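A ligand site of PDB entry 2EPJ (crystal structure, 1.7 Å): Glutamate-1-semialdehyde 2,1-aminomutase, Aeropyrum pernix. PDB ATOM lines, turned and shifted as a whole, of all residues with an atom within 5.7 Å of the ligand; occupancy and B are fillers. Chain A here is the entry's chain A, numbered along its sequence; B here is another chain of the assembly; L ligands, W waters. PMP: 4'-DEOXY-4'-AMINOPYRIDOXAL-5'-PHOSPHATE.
The side-chain hydroxyl (OG1) of Thr 122 sits at hydrogen-bond distance from an oxygen (O3P) of the ligand (2.6 Å). OG1 of Thr 303 of chain B lies within hydrogen-bond range of O1P of the ligand, at 3.0 Å. A nitrogen (N1) of the ligand sits at hydrogen-bond distance from the side-chain carboxylate (OD2) of Asp 243. O3 of the ligand lies close to NZ of Lys 271 (3.5 Å). The side-chain amide nitrogen (ND2) of Asn 215 is in hydrogen-bond range of an oxygen (O3) of the ligand (3.1 Å). N of Thr 303 of chain B is in hydrogen-bond range of O1P of the ligand, 2.8 Å away. An oxygen (O2P) of the ligand sits at hydrogen-bond distance from the backbone NH of Gly 121 (2.9 Å). O3P of the ligand sits at hydrogen-bond distance from N of Thr 122, at 2.7 Å.
The side-chain hydroxyl of Ser 120 sits at hydrogen-bond distance from the side-chain carboxylate of Glu 123 of chain B. The side-chain hydroxyl (OG1) of Thr 122 is in hydrogen-bond range of the backbone NH (N) of Ser 151, 2.8 Å away. OG of Ser 120 sits at hydrogen-bond distance from N of Glu 123 of chain A (2.9 Å). The side-chain amide nitrogen of Asn 215 lies within hydrogen-bond range of the side-chain carboxylate of Glu 210. The backbone carbonyl oxygen (O) of Phe 304 of chain B lies close to the side-chain amide oxygen (OD1) of Asn 119 of chain B, 2.8 Å away. The side-chain hydroxyl (OG1) of Thr 125 is in hydrogen-bond range of the backbone carbonyl oxygen (O) of Thr 122, 3.4 Å away. The backbone NH of Ser 120 lies close to the backbone carbonyl oxygen of Val 279 (3.3 Å). The backbone NH (N) of Thr 122 lies close to the side-chain hydroxyl (OG) of Ser 120.
N1 of the ligand lies close to O of Tyr 148, at 3.4 Å. CB of Ser 120 touches O3P of the ligand (3.6 Å). His 149 touches the ligand. N of Gly 150 touches C6 of the ligand, 3.8 Å away. Glu 210 touches the ligand. Val 245 touches the ligand (CB to N1, 3.7 Å). Val 246 touches the ligand (CG2 to O3, 3.1 Å). CA of Gly 302 of chain B touches O1P of the ligand, 3.5 Å away. Phe 304 of chain B touches the ligand (CD2 to O2P, 3.7 Å). Hydrophobic or aromatic side chains that line the ligand: Tyr 148, Val 245, Val 246 and Phe 304 of chain B. Of the 25 residues printed, 15 come within 4 Å of the ligand. The nearest printed residue that does not touch the ligand is Glu 123 of chain B (4.4 Å).
Water W3 lies within hydrogen-bond range of an oxygen (O2P) of the ligand (2.6 Å) and the side-chain hydroxyl (OG1) of Thr 303 of chain B (3.2 Å). Water W4 lies within hydrogen-bond range of an oxygen (O1P) of the ligand (2.7 Å), the side-chain hydroxyl of Tyr 148 (2.9 Å) and the backbone NH of Gly 302 of chain B (3.5 Å). Water W2 lies within hydrogen-bond range of the side-chain carboxylate of Glu 123 of chain B (2.8 Å), an oxygen (O3P) of the ligand (2.9 Å) and the side-chain amide nitrogen of Asn 119 of chain B (3.2 Å). Water W5 bridges a nitrogen (N4A) of the ligand (3.0 Å) and the side-chain amide oxygen of Asn 215 (3.2 Å).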
ATOM      1  N   ASN A 119       5.696   0.431 -18.771  1.00  0.00           N
ATOM      2  CA  ASN A 119       4.501   1.275 -18.836  1.00  0.00           C
ATOM      3  C   ASN A 119       3.781   1.537 -20.140  1.00  0.00           C
ATOM      4  O   ASN A 119       2.797   2.279 -20.185  1.00  0.00           O
ATOM      5  CB  ASN A 119       4.858   2.576 -18.140  1.00  0.00           C
ATOM      6  CG  ASN A 119       5.532   2.330 -16.814  1.00  0.00           C
ATOM      7  OD1 ASN A 119       4.870   2.017 -15.822  1.00  0.00           O
ATOM      8  ND2 ASN A 119       6.859   2.428 -16.796  1.00  0.00           N
ATOM      9  N   SER A 120       4.249   0.910 -21.210  1.00  0.00           N
ATOM     10  CA  SER A 120       3.621   1.055 -22.513  1.00  0.00           C
ATOM     11  C   SER A 120       4.147  -0.038 -23.427  1.00  0.00           C
ATOM     12  O   SER A 120       5.156  -0.676 -23.123  1.00  0.00           O
ATOM     13  CB  SER A 120       3.934   2.421 -23.126  1.00  0.00           C
ATOM     14  OG  SER A 120       5.318   2.525 -23.437  1.00  0.00           O
ATOM     15  N   GLY A 121       3.443  -0.272 -24.531  1.00  0.00           N
ATOM     16  CA  GLY A 121       3.887  -1.274 -25.480  1.00  0.00           C
ATOM     17  C   GLY A 121       5.181  -0.792 -26.105  1.00  0.00           C
ATOM     18  O   GLY A 121       6.059  -1.592 -26.438  1.00  0.00           O
ATOM     19  N   THR A 122       5.305   0.523 -26.248  1.00  0.00           N
ATOM     20  CA  THR A 122       6.500   1.146 -26.800  1.00  0.00           C
ATOM     21  C   THR A 122       7.703   0.820 -25.903  1.00  0.00           C
ATOM     22  O   THR A 122       8.746   0.392 -26.388  1.00  0.00           O
ATOM     23  CB  THR A 122       6.341   2.682 -26.907  1.00  0.00           C
ATOM     24  OG1 THR A 122       5.391   2.990 -27.936  1.00  0.00           O
ATOM     25  CG2 THR A 122       7.665   3.354 -27.230  1.00  0.00           C
ATOM     26  N   GLU A 123       7.556   1.032 -24.602  1.00  0.00           N
ATOM     27  CA  GLU A 123       8.659   0.720 -23.687  1.00  0.00           C
ATOM     28  C   GLU A 123       8.968  -0.764 -23.743  1.00  0.00           C
ATOM     29  O   GLU A 123      10.133  -1.175 -23.670  1.00  0.00           O
ATOM     30  CB  GLU A 123       8.300   1.097 -22.245  1.00  0.00           C
ATOM     31  CG  GLU A 123       8.232   2.588 -21.949  1.00  0.00           C
ATOM     32  CD  GLU A 123       8.333   2.880 -20.461  1.00  0.00           C
ATOM     33  OE1 GLU A 123       7.676   2.180 -19.667  1.00  0.00           O
ATOM     34  OE2 GLU A 123       9.086   3.811 -20.079  1.00  0.00           O
ATOM     35  N   THR A 125       8.556  -3.093 -26.326  1.00  0.00           N
ATOM     36  CA  THR A 125       9.295  -3.543 -27.499  1.00  0.00           C
ATOM     37  C   THR A 125      10.717  -2.979 -27.492  1.00  0.00           C
ATOM     38  O   THR A 125      11.655  -3.636 -27.907  1.00  0.00           O
ATOM     39  CB  THR A 125       8.583  -3.165 -28.822  1.00  0.00           C
ATOM     40  OG1 THR A 125       8.543  -1.747 -28.976  1.00  0.00           O
ATOM     41  CG2 THR A 125       7.159  -3.710 -28.814  1.00  0.00           C
ATOM     42  N   TYR A 148       3.680  -2.469 -36.531  1.00  0.00           N
ATOM     43  CA  TYR A 148       3.863  -1.321 -35.656  1.00  0.00           C
ATOM     44  C   TYR A 148       4.282  -1.844 -34.288  1.00  0.00           C
ATOM     45  O   TYR A 148       3.649  -2.735 -33.729  1.00  0.00           O
ATOM     46  CB  TYR A 148       2.548  -0.545 -35.521  1.00  0.00           C
ATOM     47  CG  TYR A 148       2.634   0.639 -34.589  1.00  0.00           C
ATOM     48  CD1 TYR A 148       3.424   1.738 -34.897  1.00  0.00           C
ATOM     49  CD2 TYR A 148       1.939   0.642 -33.373  1.00  0.00           C
ATOM     50  CE1 TYR A 148       3.515   2.830 -34.026  1.00  0.00           C
ATOM     51  CE2 TYR A 148       2.026   1.726 -32.491  1.00  0.00           C
ATOM     52  CZ  TYR A 148       2.821   2.816 -32.841  1.00  0.00           C
ATOM     53  OH  TYR A 148       2.914   3.889 -31.985  1.00  0.00           O
ATOM     54  N   HIS A 149       5.368  -1.281 -33.756  1.00  0.00           N
ATOM     55  CA  HIS A 149       5.877  -1.708 -32.466  1.00  0.00           C
ATOM     56  C   HIS A 149       6.009  -0.574 -31.462  1.00  0.00           C
ATOM     57  O   HIS A 149       6.632  -0.734 -30.406  1.00  0.00           O
ATOM     58  CB  HIS A 149       7.240  -2.400 -32.667  1.00  0.00           C
ATOM     59  CG  HIS A 149       7.189  -3.525 -33.633  1.00  0.00           C
ATOM     60  ND1 HIS A 149       6.403  -4.644 -33.433  1.00  0.00           N
ATOM     61  CD2 HIS A 149       7.785  -3.700 -34.835  1.00  0.00           C
ATOM     62  CE1 HIS A 149       6.518  -5.451 -34.471  1.00  0.00           C
ATOM     63  NE2 HIS A 149       7.350  -4.907 -35.338  1.00  0.00           N
ATOM     64  N   GLY A 150       5.402   0.557 -31.759  1.00  0.00           N
ATOM     65  CA  GLY A 150       5.490   1.656 -30.828  1.00  0.00           C
ATOM     66  C   GLY A 150       6.225   2.881 -31.331  1.00  0.00           C
ATOM     67  O   GLY A 150       6.703   2.922 -32.465  1.00  0.00           O
ATOM     68  N   SER A 151       6.337   3.860 -30.437  1.00  0.00           N
ATOM     69  CA  SER A 151       6.947   5.128 -30.757  1.00  0.00           C
ATOM     70  C   SER A 151       8.408   5.304 -30.325  1.00  0.00           C
ATOM     71  O   SER A 151       8.728   6.195 -29.542  1.00  0.00           O
ATOM     72  CB  SER A 151       6.080   6.245 -30.144  1.00  0.00           C
ATOM     73  OG  SER A 151       6.494   7.535 -30.551  1.00  0.00           O
ATOM     74  N   GLU A 210       4.487  -8.943 -35.428  1.00  0.00           N
ATOM     75  CA  GLU A 210       3.156  -9.091 -34.857  1.00  0.00           C
ATOM     76  C   GLU A 210       2.634 -10.393 -35.440  1.00  0.00           C
ATOM     77  O   GLU A 210       2.618 -10.560 -36.656  1.00  0.00           O
ATOM     78  CB  GLU A 210       2.219  -7.963 -35.314  1.00  0.00           C
ATOM     79  CG  GLU A 210       2.491  -6.593 -34.737  1.00  0.00           C
ATOM     80  CD  GLU A 210       1.616  -5.524 -35.375  1.00  0.00           C
ATOM     81  OE1 GLU A 210       0.413  -5.434 -35.039  1.00  0.00           O
ATOM     82  OE2 GLU A 210       2.129  -4.779 -36.237  1.00  0.00           O
ATOM     83  N   ALA A 214      -2.120  -5.670 -36.712  1.00  0.00           N
ATOM     84  CA  ALA A 214      -3.304  -4.956 -36.236  1.00  0.00           C
ATOM     85  C   ALA A 214      -3.246  -3.473 -36.555  1.00  0.00           C
ATOM     86  O   ALA A 214      -4.199  -2.743 -36.287  1.00  0.00           O
ATOM     87  CB  ALA A 214      -3.443  -5.154 -34.727  1.00  0.00           C
ATOM     88  N   ASN A 215      -2.142  -3.023 -37.145  1.00  0.00           N
ATOM     89  CA  ASN A 215      -1.967  -1.608 -37.463  1.00  0.00           C
ATOM     90  C   ASN A 215      -1.770  -1.283 -38.944  1.00  0.00           C
ATOM     91  O   ASN A 215      -1.222  -0.234 -39.300  1.00  0.00           O
ATOM     92  CB  ASN A 215      -0.822  -1.054 -36.614  1.00  0.00           C
ATOM     93  CG  ASN A 215      -1.049  -1.264 -35.120  1.00  0.00           C
ATOM     94  OD1 ASN A 215      -1.820  -0.537 -34.494  1.00  0.00           O
ATOM     95  ND2 ASN A 215      -0.382  -2.268 -34.550  1.00  0.00           N
ATOM     96  N   ASP A 243       5.749  -9.762 -30.961  1.00  0.00           N
ATOM     97  CA  ASP A 243       5.101  -8.595 -30.392  1.00  0.00           C
ATOM     98  C   ASP A 243       3.629  -8.956 -30.232  1.00  0.00           C
ATOM     99  O   ASP A 243       2.858  -8.870 -31.185  1.00  0.00           O
ATOM    100  CB  ASP A 243       5.258  -7.368 -31.286  1.00  0.00           C
ATOM    101  CG  ASP A 243       4.631  -6.129 -30.673  1.00  0.00           C
ATOM    102  OD1 ASP A 243       3.859  -6.270 -29.702  1.00  0.00           O
ATOM    103  OD2 ASP A 243       4.898  -5.008 -31.156  1.00  0.00           O
ATOM    104  N   GLU A 244       3.274  -9.384 -29.033  1.00  0.00           N
ATOM    105  CA  GLU A 244       1.912  -9.771 -28.718  1.00  0.00           C
ATOM    106  C   GLU A 244       1.206  -8.707 -27.887  1.00  0.00           C
ATOM    107  O   GLU A 244       0.345  -9.020 -27.066  1.00  0.00           O
ATOM    108  CB  GLU A 244       1.890 -11.098 -27.962  1.00  0.00           C
ATOM    109  CG  GLU A 244       2.351 -12.289 -28.800  1.00  0.00           C
ATOM    110  CD  GLU A 244       1.547 -13.541 -28.514  1.00  0.00           C
ATOM    111  OE1 GLU A 244       0.299 -13.456 -28.509  1.00  0.00           O
ATOM    112  OE2 GLU A 244       2.161 -14.618 -28.303  1.00  0.00           O
ATOM    113  N   VAL A 245       1.563  -7.453 -28.109  1.00  0.00           N
ATOM    114  CA  VAL A 245       0.931  -6.360 -27.377  1.00  0.00           C
ATOM    115  C   VAL A 245      -0.574  -6.400 -27.634  1.00  0.00           C
ATOM    116  O   VAL A 245      -1.368  -6.104 -26.744  1.00  0.00           O
ATOM    117  CB  VAL A 245       1.547  -5.002 -27.784  1.00  0.00           C
ATOM    118  CG1 VAL A 245       0.667  -3.850 -27.299  1.00  0.00           C
ATOM    119  CG2 VAL A 245       2.930  -4.881 -27.163  1.00  0.00           C
ATOM    120  N   VAL A 246      -0.964  -6.768 -28.862  1.00  0.00           N
ATOM    121  CA  VAL A 246      -2.382  -6.875 -29.204  1.00  0.00           C
ATOM    122  C   VAL A 246      -2.906  -8.317 -29.118  1.00  0.00           C
ATOM    123  O   VAL A 246      -3.956  -8.566 -28.518  1.00  0.00           O
ATOM    124  CB  VAL A 246      -2.666  -6.340 -30.641  1.00  0.00           C
ATOM    125  CG1 VAL A 246      -4.076  -6.729 -31.079  1.00  0.00           C
ATOM    126  CG2 VAL A 246      -2.510  -4.829 -30.675  1.00  0.00           C
ATOM    127  N   LYS A 271      -1.374  -3.792 -23.529  1.00  0.00           N
ATOM    128  CA  LYS A 271      -2.817  -3.570 -23.604  1.00  0.00           C
ATOM    129  C   LYS A 271      -3.664  -4.374 -22.618  1.00  0.00           C
ATOM    130  O   LYS A 271      -3.809  -3.975 -21.470  1.00  0.00           O
ATOM    131  CB  LYS A 271      -3.278  -3.779 -25.044  1.00  0.00           C
ATOM    132  CG  LYS A 271      -2.668  -2.738 -25.983  1.00  0.00           C
ATOM    133  CD  LYS A 271      -3.196  -2.835 -27.409  1.00  0.00           C
ATOM    134  CE  LYS A 271      -2.771  -1.604 -28.205  1.00  0.00           C
ATOM    135  NZ  LYS A 271      -3.195  -1.639 -29.627  1.00  0.00           N
ATOM    136  N   VAL A 279       0.524   0.040 -19.382  1.00  0.00           N
ATOM    137  CA  VAL A 279       1.272  -1.191 -19.182  1.00  0.00           C
ATOM    138  C   VAL A 279       2.038  -1.664 -20.419  1.00  0.00           C
ATOM    139  O   VAL A 279       1.772  -1.247 -21.548  1.00  0.00           O
ATOM    140  CB  VAL A 279       0.314  -2.335 -18.750  1.00  0.00           C
ATOM    141  CG1 VAL A 279      -0.533  -2.781 -19.943  1.00  0.00           C
ATOM    142  CG2 VAL A 279       1.099  -3.511 -18.164  1.00  0.00           C
ATOM    143  N   ASN B 119       3.560   8.294 -21.237  1.00  0.00           N
ATOM    144  CA  ASN B 119       3.376   7.419 -20.078  1.00  0.00           C
ATOM    145  C   ASN B 119       4.493   7.172 -19.078  1.00  0.00           C
ATOM    146  O   ASN B 119       4.328   6.397 -18.133  1.00  0.00           O
ATOM    147  CB  ASN B 119       2.816   6.113 -20.613  1.00  0.00           C
ATOM    148  CG  ASN B 119       1.671   6.348 -21.567  1.00  0.00           C
ATOM    149  OD1 ASN B 119       0.546   6.619 -21.142  1.00  0.00           O
ATOM    150  ND2 ASN B 119       1.959   6.287 -22.864  1.00  0.00           N
ATOM    151  N   GLU B 123       9.676   7.876 -21.729  1.00  0.00           N
ATOM    152  CA  GLU B 123       9.028   8.199 -23.004  1.00  0.00           C
ATOM    153  C   GLU B 123       9.110   9.692 -23.259  1.00  0.00           C
ATOM    154  O   GLU B 123       9.293  10.134 -24.400  1.00  0.00           O
ATOM    155  CB  GLU B 123       7.553   7.780 -22.993  1.00  0.00           C
ATOM    156  CG  GLU B 123       7.292   6.281 -23.028  1.00  0.00           C
ATOM    157  CD  GLU B 123       5.875   5.959 -23.472  1.00  0.00           C
ATOM    158  OE1 GLU B 123       4.938   6.628 -22.992  1.00  0.00           O
ATOM    159  OE2 GLU B 123       5.701   5.042 -24.314  1.00  0.00           O
ATOM    160  N   ALA B 301       2.993   8.560 -30.654  1.00  0.00           N
ATOM    161  CA  ALA B 301       1.658   8.020 -30.487  1.00  0.00           C
ATOM    162  C   ALA B 301       1.717   7.153 -29.246  1.00  0.00           C
ATOM    163  O   ALA B 301       2.789   6.709 -28.840  1.00  0.00           O
ATOM    164  CB  ALA B 301       1.282   7.183 -31.709  1.00  0.00           C
ATOM    165  N   GLY B 302       0.570   6.910 -28.622  1.00  0.00           N
ATOM    166  CA  GLY B 302       0.561   6.093 -27.434  1.00  0.00           C
ATOM    167  C   GLY B 302      -0.854   5.714 -27.040  1.00  0.00           C
ATOM    168  O   GLY B 302      -1.697   6.580 -26.839  1.00  0.00           O
ATOM    169  N   THR B 303      -1.086   4.415 -26.936  1.00  0.00           N
ATOM    170  CA  THR B 303      -2.390   3.883 -26.552  1.00  0.00           C
ATOM    171  C   THR B 303      -2.847   4.508 -25.226  1.00  0.00           C
ATOM    172  O   THR B 303      -4.024   4.836 -25.060  1.00  0.00           O
ATOM    173  CB  THR B 303      -2.313   2.350 -26.370  1.00  0.00           C
ATOM    174  OG1 THR B 303      -1.922   1.747 -27.602  1.00  0.00           O
ATOM    175  CG2 THR B 303      -3.657   1.785 -25.925  1.00  0.00           C
ATOM    176  N   PHE B 304      -1.904   4.707 -24.320  1.00  0.00           N
ATOM    177  CA  PHE B 304      -2.220   5.250 -23.014  1.00  0.00           C
ATOM    178  C   PHE B 304      -1.945   6.746 -22.816  1.00  0.00           C
ATOM    179  O   PHE B 304      -2.165   7.275 -21.726  1.00  0.00           O
ATOM    180  CB  PHE B 304      -1.491   4.425 -21.940  1.00  0.00           C
ATOM    181  CG  PHE B 304      -1.836   2.957 -21.984  1.00  0.00           C
ATOM    182  CD1 PHE B 304      -3.134   2.532 -21.702  1.00  0.00           C
ATOM    183  CD2 PHE B 304      -0.877   2.015 -22.331  1.00  0.00           C
ATOM    184  CE1 PHE B 304      -3.471   1.181 -21.764  1.00  0.00           C
ATOM    185  CE2 PHE B 304      -1.207   0.649 -22.401  1.00  0.00           C
ATOM    186  CZ  PHE B 304      -2.504   0.239 -22.116  1.00  0.00           C
HETATM  187  N1  PMP L   1       3.024  -2.953 -30.434  1.00  0.00           N
HETATM  188  C2  PMP L   1       1.850  -3.272 -31.007  1.00  0.00           C
HETATM  189  C2A PMP L   1       1.683  -4.576 -31.754  1.00  0.00           C
HETATM  190  C3  PMP L   1       0.747  -2.379 -30.923  1.00  0.00           C
HETATM  191  O3  PMP L   1      -0.451  -2.682 -31.493  1.00  0.00           O
HETATM  192  C4  PMP L   1       0.911  -1.167 -30.230  1.00  0.00           C
HETATM  193  C4A PMP L   1      -0.257  -0.188 -30.113  1.00  0.00           C
HETATM  194  N4A PMP L   1      -0.643   0.312 -31.439  1.00  0.00           N
HETATM  195  C5  PMP L   1       2.171  -0.868 -29.630  1.00  0.00           C
HETATM  196  C6  PMP L   1       3.228  -1.793 -29.756  1.00  0.00           C
HETATM  197  C5A PMP L   1       2.285   0.451 -28.901  1.00  0.00           C
HETATM  198  O4P PMP L   1       1.760   0.252 -27.589  1.00  0.00           O
HETATM  199  P   PMP L   1       1.806   1.645 -26.781  1.00  0.00           P
HETATM  200  O1P PMP L   1       0.928   2.591 -27.508  1.00  0.00           O
HETATM  201  O2P PMP L   1       1.222   1.399 -25.304  1.00  0.00           O
HETATM  202  O3P PMP L   1       3.275   2.256 -26.682  1.00  0.00           O
HETATM  203  O   HOH W   1       0.752   3.811 -24.377  1.00  0.00           O
HETATM  204  O   HOH W   2       3.212   4.943 -25.524  1.00  0.00           O
HETATM  205  O   HOH W   3      -0.438  -0.538 -25.989  1.00  0.00           O
HETATM  206  O   HOH W   4       0.849   3.717 -29.989  1.00  0.00           O
HETATM  207  O   HOH W   5      -3.178   1.443 -32.447  1.00  0.00           O
